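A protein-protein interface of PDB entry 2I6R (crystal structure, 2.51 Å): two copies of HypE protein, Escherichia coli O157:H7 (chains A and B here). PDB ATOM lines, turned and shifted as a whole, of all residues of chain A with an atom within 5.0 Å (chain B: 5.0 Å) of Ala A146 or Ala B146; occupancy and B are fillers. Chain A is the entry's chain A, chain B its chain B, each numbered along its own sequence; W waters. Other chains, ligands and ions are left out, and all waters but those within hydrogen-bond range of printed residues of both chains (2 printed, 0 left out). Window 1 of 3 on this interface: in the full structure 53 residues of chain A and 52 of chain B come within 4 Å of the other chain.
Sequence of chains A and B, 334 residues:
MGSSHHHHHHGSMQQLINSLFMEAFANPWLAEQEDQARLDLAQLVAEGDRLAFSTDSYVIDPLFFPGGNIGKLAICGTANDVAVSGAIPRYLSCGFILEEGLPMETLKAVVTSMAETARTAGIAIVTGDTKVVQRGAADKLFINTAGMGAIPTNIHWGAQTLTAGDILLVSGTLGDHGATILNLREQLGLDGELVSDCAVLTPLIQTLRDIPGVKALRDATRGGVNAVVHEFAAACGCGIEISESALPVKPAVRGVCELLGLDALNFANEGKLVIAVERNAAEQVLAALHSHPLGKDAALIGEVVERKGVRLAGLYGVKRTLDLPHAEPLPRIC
OD1 of Asn B144 sits close to OD1 of Asn A144.
Phe A53 touches Met B148, and with the chains exchanged Met A148 touches Phe B53.
Thr A55 touches Ser B93, and with the chains exchanged Ser A93 touches Thr B55.
Asn B144 touches its own counterpart, Asn A144.
Ala B146 touches its own counterpart, Ala A146.
12 positions are printed for both chains.
Of the 8 pairs that touch across the chains among the printed residues, 8 have their exchanged pair printed and touching as well.
O of Tyr A91 is in hydrogen-bond range of N of Met A148, at 3.1 Å.
O of Thr B145 lies within hydrogen-bond range of OG1 of Thr B55, at 3.1 Å.
The side-chain hydroxyl of Thr B55 is in hydrogen-bond range of the side-chain amide oxygen of Asn B144 (3.1 Å).
The backbone carbonyl oxygen (O) of Thr A145 is in hydrogen-bond range of the side-chain hydroxyl (OG1) of Thr A55, at 3.1 Å.
The side-chain amide oxygen (OD1) of Asn A144 lies within hydrogen-bond range of the side-chain hydroxyl (OG1) of Thr A55 (3.1 Å).
O of Ala B146 is in hydrogen-bond range of N of Ser B93 (2.7 Å).
Among the printed residues, pairs that only touch across the chains: Ser A93 with Phe B53, Phe A53 with Ser B93, Phe A53 with Met B148, Ser A93 with Thr B55, Met A148 with Phe B53, Thr A55 with Ser B93 and Ala A146 with Ala B146.
Printed residues of chain B within 4 Å of Phe A53: Ser B93 and Met B148.
Of the printed residues of chain B, Ser A93 touches Phe B53 (3.3 Å) and Thr B55 (3.7 Å).
Of the printed residues of chain B, Ala A146 touches Ala B146.
Ala B146 touches just one residue of chain A: Ala A146 (3.9 Å).
The nearest printed residue of chain B that does not touch Met A148 is Met B148 (4.1 Å).
Hydrophobic or aromatic side chains of chain B that line the printed part of chain A: Phe B53, Ala B146 and Met B148.
Along chain B the printed residues that touch a printed residue of chain A span positions 53 to 148.
Hydrophobic or aromatic side chains of chain A that line the printed part of chain B: Phe A53, Ala A146 and Met A148.
Among the printed residues, no Asp or Glu carboxylate lies within 4 Å of a Lys or Arg side-chain nitrogen of the other chain.
Water W2 lies within hydrogen-bond range of the side-chain hydroxyl (OG) of Ser B93, the side-chain hydroxyl (OG1) of Thr A55, the side-chain amide oxygen (OD1) of Asn B144 and the side-chain amide oxygen (OD1) of Asn A144.
Water W1 lies within hydrogen-bond range of the side-chain hydroxyl (OG1) of Thr B55 (2.7 Å), the side-chain hydroxyl (OG) of Ser A93 (3.0 Å), the side-chain amide oxygen (OD1) of Asn A144 (3.0 Å) and the side-chain amide oxygen (OD1) of Asn B144 (3.2 Å).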
ATOM      1  N   PHE A  53      -7.939 -14.479  27.265  1.00  0.00           N
ATOM      2  CA  PHE A  53      -7.447 -15.545  26.412  1.00  0.00           C
ATOM      3  C   PHE A  53      -6.709 -16.573  27.258  1.00  0.00           C
ATOM      4  O   PHE A  53      -5.748 -16.248  27.938  1.00  0.00           O
ATOM      5  CB  PHE A  53      -6.557 -14.944  25.320  1.00  0.00           C
ATOM      6  CG  PHE A  53      -5.967 -15.950  24.381  1.00  0.00           C
ATOM      7  CD1 PHE A  53      -6.766 -16.905  23.759  1.00  0.00           C
ATOM      8  CD2 PHE A  53      -4.610 -15.918  24.086  1.00  0.00           C
ATOM      9  CE1 PHE A  53      -6.219 -17.830  22.880  1.00  0.00           C
ATOM     10  CE2 PHE A  53      -4.052 -16.839  23.198  1.00  0.00           C
ATOM     11  CZ  PHE A  53      -4.861 -17.794  22.596  1.00  0.00           C
ATOM     12  N   SER A  54      -7.180 -17.813  27.229  1.00  0.00           N
ATOM     13  CA  SER A  54      -6.588 -18.847  28.054  1.00  0.00           C
ATOM     14  C   SER A  54      -6.433 -20.179  27.331  1.00  0.00           C
ATOM     15  O   SER A  54      -7.152 -20.463  26.388  1.00  0.00           O
ATOM     16  CB  SER A  54      -7.433 -19.043  29.296  1.00  0.00           C
ATOM     17  OG  SER A  54      -6.719 -19.829  30.237  1.00  0.00           O
ATOM     18  N   THR A  55      -5.501 -21.002  27.795  1.00  0.00           N
ATOM     19  CA  THR A  55      -5.358 -22.350  27.275  1.00  0.00           C
ATOM     20  C   THR A  55      -5.021 -23.360  28.358  1.00  0.00           C
ATOM     21  O   THR A  55      -4.412 -23.028  29.369  1.00  0.00           O
ATOM     22  CB  THR A  55      -4.290 -22.450  26.170  1.00  0.00           C
ATOM     23  OG1 THR A  55      -4.378 -23.743  25.552  1.00  0.00           O
ATOM     24  CG2 THR A  55      -2.883 -22.249  26.736  1.00  0.00           C
ATOM     25  N   THR A  78     -11.225 -24.476  30.714  1.00  0.00           N
ATOM     26  CA  THR A  78     -10.898 -23.329  29.882  1.00  0.00           C
ATOM     27  C   THR A  78     -11.968 -22.251  29.972  1.00  0.00           C
ATOM     28  O   THR A  78     -11.649 -21.062  30.100  1.00  0.00           O
ATOM     29  CB  THR A  78     -10.628 -23.748  28.436  1.00  0.00           C
ATOM     30  OG1 THR A  78      -9.474 -24.596  28.424  1.00  0.00           O
ATOM     31  CG2 THR A  78     -10.374 -22.535  27.555  1.00  0.00           C
ATOM     32  N   TYR A  91     -15.951 -18.233  22.615  1.00  0.00           N
ATOM     33  CA  TYR A  91     -15.343 -19.054  21.577  1.00  0.00           C
ATOM     34  C   TYR A  91     -14.223 -19.944  22.088  1.00  0.00           C
ATOM     35  O   TYR A  91     -13.342 -19.488  22.815  1.00  0.00           O
ATOM     36  CB  TYR A  91     -14.790 -18.167  20.475  1.00  0.00           C
ATOM     37  CG  TYR A  91     -15.767 -17.171  19.917  1.00  0.00           C
ATOM     38  CD1 TYR A  91     -15.498 -15.806  19.971  1.00  0.00           C
ATOM     39  CD2 TYR A  91     -16.956 -17.588  19.327  1.00  0.00           C
ATOM     40  CE1 TYR A  91     -16.385 -14.880  19.437  1.00  0.00           C
ATOM     41  CE2 TYR A  91     -17.858 -16.673  18.805  1.00  0.00           C
ATOM     42  CZ  TYR A  91     -17.560 -15.321  18.860  1.00  0.00           C
ATOM     43  OH  TYR A  91     -18.440 -14.419  18.339  1.00  0.00           O
ATOM     44  N   LEU A  92     -14.262 -21.207  21.678  1.00  0.00           N
ATOM     45  CA  LEU A  92     -13.284 -22.213  22.068  1.00  0.00           C
ATOM     46  C   LEU A  92     -12.619 -22.836  20.861  1.00  0.00           C
ATOM     47  O   LEU A  92     -13.261 -23.076  19.850  1.00  0.00           O
ATOM     48  CB  LEU A  92     -13.970 -23.318  22.869  1.00  0.00           C
ATOM     49  CG  LEU A  92     -13.972 -23.308  24.406  1.00  0.00           C
ATOM     50  CD1 LEU A  92     -13.006 -24.332  24.938  1.00  0.00           C
ATOM     51  CD2 LEU A  92     -13.686 -21.943  25.014  1.00  0.00           C
ATOM     52  N   SER A  93     -11.323 -23.100  20.974  1.00  0.00           N
ATOM     53  CA  SER A  93     -10.614 -23.927  20.006  1.00  0.00           C
ATOM     54  C   SER A  93     -10.295 -25.235  20.689  1.00  0.00           C
ATOM     55  O   SER A  93     -10.312 -25.315  21.916  1.00  0.00           O
ATOM     56  CB  SER A  93      -9.320 -23.265  19.538  1.00  0.00           C
ATOM     57  OG  SER A  93      -8.296 -23.408  20.504  1.00  0.00           O
ATOM     58  N   ASN A 144      -6.363 -30.468  24.205  1.00  0.00           N
ATOM     59  CA  ASN A 144      -6.102 -29.085  24.540  1.00  0.00           C
ATOM     60  C   ASN A 144      -7.249 -28.198  24.080  1.00  0.00           C
ATOM     61  O   ASN A 144      -7.719 -28.317  22.951  1.00  0.00           O
ATOM     62  CB  ASN A 144      -4.782 -28.597  23.950  1.00  0.00           C
ATOM     63  CG  ASN A 144      -4.460 -27.156  24.364  1.00  0.00           C
ATOM     64  OD1 ASN A 144      -5.008 -26.200  23.798  1.00  0.00           O
ATOM     65  ND2 ASN A 144      -3.583 -26.995  25.367  1.00  0.00           N
ATOM     66  N   THR A 145      -7.707 -27.322  24.966  1.00  0.00           N
ATOM     67  CA  THR A 145      -8.630 -26.273  24.576  1.00  0.00           C
ATOM     68  C   THR A 145      -8.050 -24.901  24.892  1.00  0.00           C
ATOM     69  O   THR A 145      -7.284 -24.741  25.838  1.00  0.00           O
ATOM     70  CB  THR A 145     -10.009 -26.401  25.252  1.00  0.00           C
ATOM     71  OG1 THR A 145      -9.866 -26.277  26.673  1.00  0.00           O
ATOM     72  CG2 THR A 145     -10.690 -27.732  24.908  1.00  0.00           C
ATOM     73  N   ALA A 146      -8.435 -23.922  24.083  1.00  0.00           N
ATOM     74  CA  ALA A 146      -8.059 -22.532  24.244  1.00  0.00           C
ATOM     75  C   ALA A 146      -9.328 -21.722  24.048  1.00  0.00           C
ATOM     76  O   ALA A 146     -10.174 -22.087  23.232  1.00  0.00           O
ATOM     77  CB  ALA A 146      -7.010 -22.140  23.225  1.00  0.00           C
ATOM     78  N   GLY A 147      -9.468 -20.626  24.792  1.00  0.00           N
ATOM     79  CA  GLY A 147     -10.732 -19.912  24.827  1.00  0.00           C
ATOM     80  C   GLY A 147     -10.611 -18.429  25.044  1.00  0.00           C
ATOM     81  O   GLY A 147      -9.581 -17.935  25.516  1.00  0.00           O
ATOM     82  N   MET A 148     -11.676 -17.713  24.703  1.00  0.00           N
ATOM     83  CA  MET A 148     -11.675 -16.254  24.807  1.00  0.00           C
ATOM     84  C   MET A 148     -13.053 -15.688  25.088  1.00  0.00           C
ATOM     85  O   MET A 148     -14.083 -16.295  24.761  1.00  0.00           O
ATOM     86  CB  MET A 148     -11.095 -15.599  23.544  1.00  0.00           C
ATOM     87  CG  MET A 148     -11.984 -15.728  22.318  1.00  0.00           C
ATOM     88  SD  MET A 148     -11.229 -15.099  20.801  1.00  0.00           S
ATOM     89  CE  MET A 148     -10.010 -16.385  20.438  1.00  0.00           C
ATOM     90  N   PHE B  53      -8.379 -16.931  14.135  1.00  0.00           N
ATOM     91  CA  PHE B  53      -8.096 -17.749  15.293  1.00  0.00           C
ATOM     92  C   PHE B  53      -7.897 -19.188  14.826  1.00  0.00           C
ATOM     93  O   PHE B  53      -8.794 -19.805  14.226  1.00  0.00           O
ATOM     94  CB  PHE B  53      -9.252 -17.626  16.294  1.00  0.00           C
ATOM     95  CG  PHE B  53      -9.094 -18.458  17.552  1.00  0.00           C
ATOM     96  CD1 PHE B  53      -7.895 -18.486  18.257  1.00  0.00           C
ATOM     97  CD2 PHE B  53     -10.181 -19.180  18.055  1.00  0.00           C
ATOM     98  CE1 PHE B  53      -7.761 -19.251  19.435  1.00  0.00           C
ATOM     99  CE2 PHE B  53     -10.068 -19.943  19.236  1.00  0.00           C
ATOM    100  CZ  PHE B  53      -8.848 -19.974  19.929  1.00  0.00           C
ATOM    101  N   SER B  54      -6.712 -19.717  15.101  1.00  0.00           N
ATOM    102  CA  SER B  54      -6.393 -21.074  14.712  1.00  0.00           C
ATOM    103  C   SER B  54      -5.698 -21.832  15.813  1.00  0.00           C
ATOM    104  O   SER B  54      -5.093 -21.234  16.702  1.00  0.00           O
ATOM    105  CB  SER B  54      -5.502 -21.079  13.482  1.00  0.00           C
ATOM    106  OG  SER B  54      -5.431 -22.409  12.964  1.00  0.00           O
ATOM    107  N   THR B  55      -5.773 -23.154  15.734  1.00  0.00           N
ATOM    108  CA  THR B  55      -5.076 -24.020  16.667  1.00  0.00           C
ATOM    109  C   THR B  55      -4.526 -25.265  15.973  1.00  0.00           C
ATOM    110  O   THR B  55      -5.145 -25.801  15.060  1.00  0.00           O
ATOM    111  CB  THR B  55      -5.989 -24.438  17.844  1.00  0.00           C
ATOM    112  OG1 THR B  55      -5.186 -25.033  18.865  1.00  0.00           O
ATOM    113  CG2 THR B  55      -7.046 -25.441  17.405  1.00  0.00           C
ATOM    114  N   THR B  78       0.975 -22.647  13.331  1.00  0.00           N
ATOM    115  CA  THR B  78      -0.138 -21.867  13.847  1.00  0.00           C
ATOM    116  C   THR B  78      -0.080 -20.430  13.332  1.00  0.00           C
ATOM    117  O   THR B  78      -1.117 -19.864  12.962  1.00  0.00           O
ATOM    118  CB  THR B  78      -0.163 -21.920  15.386  1.00  0.00           C
ATOM    119  OG1 THR B  78      -0.403 -23.271  15.786  1.00  0.00           O
ATOM    120  CG2 THR B  78      -1.271 -21.040  15.963  1.00  0.00           C
ATOM    121  N   TYR B  91      -0.546 -12.804  18.677  1.00  0.00           N
ATOM    122  CA  TYR B  91      -0.556 -13.468  19.990  1.00  0.00           C
ATOM    123  C   TYR B  91      -0.755 -14.965  19.873  1.00  0.00           C
ATOM    124  O   TYR B  91      -1.587 -15.441  19.100  1.00  0.00           O
ATOM    125  CB  TYR B  91      -1.639 -12.913  20.920  1.00  0.00           C
ATOM    126  CG  TYR B  91      -1.670 -11.413  21.056  1.00  0.00           C
ATOM    127  CD1 TYR B  91      -2.810 -10.690  20.695  1.00  0.00           C
ATOM    128  CD2 TYR B  91      -0.567 -10.714  21.549  1.00  0.00           C
ATOM    129  CE1 TYR B  91      -2.847  -9.313  20.819  1.00  0.00           C
ATOM    130  CE2 TYR B  91      -0.592  -9.343  21.674  1.00  0.00           C
ATOM    131  CZ  TYR B  91      -1.732  -8.643  21.311  1.00  0.00           C
ATOM    132  OH  TYR B  91      -1.757  -7.273  21.433  1.00  0.00           O
ATOM    133  N   LEU B  92      -0.027 -15.695  20.700  1.00  0.00           N
ATOM    134  CA  LEU B  92       0.000 -17.127  20.620  1.00  0.00           C
ATOM    135  C   LEU B  92      -0.096 -17.763  22.003  1.00  0.00           C
ATOM    136  O   LEU B  92       0.474 -17.267  22.976  1.00  0.00           O
ATOM    137  CB  LEU B  92       1.287 -17.518  19.925  1.00  0.00           C
ATOM    138  CG  LEU B  92       1.318 -18.885  19.282  1.00  0.00           C
ATOM    139  CD1 LEU B  92       1.924 -18.787  17.899  1.00  0.00           C
ATOM    140  CD2 LEU B  92       2.105 -19.825  20.195  1.00  0.00           C
ATOM    141  N   SER B  93      -0.851 -18.849  22.088  1.00  0.00           N
ATOM    142  CA  SER B  93      -0.961 -19.613  23.319  1.00  0.00           C
ATOM    143  C   SER B  93      -0.205 -20.896  23.104  1.00  0.00           C
ATOM    144  O   SER B  93      -0.070 -21.349  21.979  1.00  0.00           O
ATOM    145  CB  SER B  93      -2.414 -19.935  23.650  1.00  0.00           C
ATOM    146  OG  SER B  93      -2.882 -21.025  22.868  1.00  0.00           O
ATOM    147  N   ASN B 144       0.656 -28.090  21.812  1.00  0.00           N
ATOM    148  CA  ASN B 144      -0.439 -27.372  21.148  1.00  0.00           C
ATOM    149  C   ASN B 144      -0.211 -25.864  21.158  1.00  0.00           C
ATOM    150  O   ASN B 144       0.206 -25.296  22.167  1.00  0.00           O
ATOM    151  CB  ASN B 144      -1.803 -27.673  21.768  1.00  0.00           C
ATOM    152  CG  ASN B 144      -2.962 -26.979  21.007  1.00  0.00           C
ATOM    153  OD1 ASN B 144      -3.204 -25.773  21.171  1.00  0.00           O
ATOM    154  ND2 ASN B 144      -3.671 -27.744  20.171  1.00  0.00           N
ATOM    155  N   THR B 145      -0.496 -25.217  20.032  1.00  0.00           N
ATOM    156  CA  THR B 145      -0.543 -23.770  19.984  1.00  0.00           C
ATOM    157  C   THR B 145      -1.841 -23.274  19.363  1.00  0.00           C
ATOM    158  O   THR B 145      -2.365 -23.863  18.413  1.00  0.00           O
ATOM    159  CB  THR B 145       0.678 -23.140  19.249  1.00  0.00           C
ATOM    160  OG1 THR B 145       0.825 -23.722  17.952  1.00  0.00           O
ATOM    161  CG2 THR B 145       1.966 -23.350  20.033  1.00  0.00           C
ATOM    162  N   ALA B 146      -2.359 -22.189  19.922  1.00  0.00           N
ATOM    163  CA  ALA B 146      -3.434 -21.440  19.304  1.00  0.00           C
ATOM    164  C   ALA B 146      -2.914 -20.025  19.059  1.00  0.00           C
ATOM    165  O   ALA B 146      -2.020 -19.565  19.767  1.00  0.00           O
ATOM    166  CB  ALA B 146      -4.669 -21.438  20.181  1.00  0.00           C
ATOM    167  N   GLY B 147      -3.435 -19.352  18.037  1.00  0.00           N
ATOM    168  CA  GLY B 147      -2.886 -18.065  17.645  1.00  0.00           C
ATOM    169  C   GLY B 147      -3.934 -17.162  17.035  1.00  0.00           C
ATOM    170  O   GLY B 147      -4.977 -17.633  16.586  1.00  0.00           O
ATOM    171  N   MET B 148      -3.646 -15.864  17.003  1.00  0.00           N
ATOM    172  CA  MET B 148      -4.605 -14.895  16.498  1.00  0.00           C
ATOM    173  C   MET B 148      -3.955 -13.657  15.887  1.00  0.00           C
ATOM    174  O   MET B 148      -2.813 -13.294  16.206  1.00  0.00           O
ATOM    175  CB  MET B 148      -5.621 -14.504  17.585  1.00  0.00           C
ATOM    176  CG  MET B 148      -5.026 -13.730  18.740  1.00  0.00           C
ATOM    177  SD  MET B 148      -6.212 -13.253  20.008  1.00  0.00           S
ATOM    178  CE  MET B 148      -6.332 -14.755  20.973  1.00  0.00           C
HETATM  179  O   HOH W   1      -6.424 -25.587  21.201  1.00  0.00           O
HETATM  180  O   HOH W   2      -2.744 -23.576  23.331  1.00  0.00           O
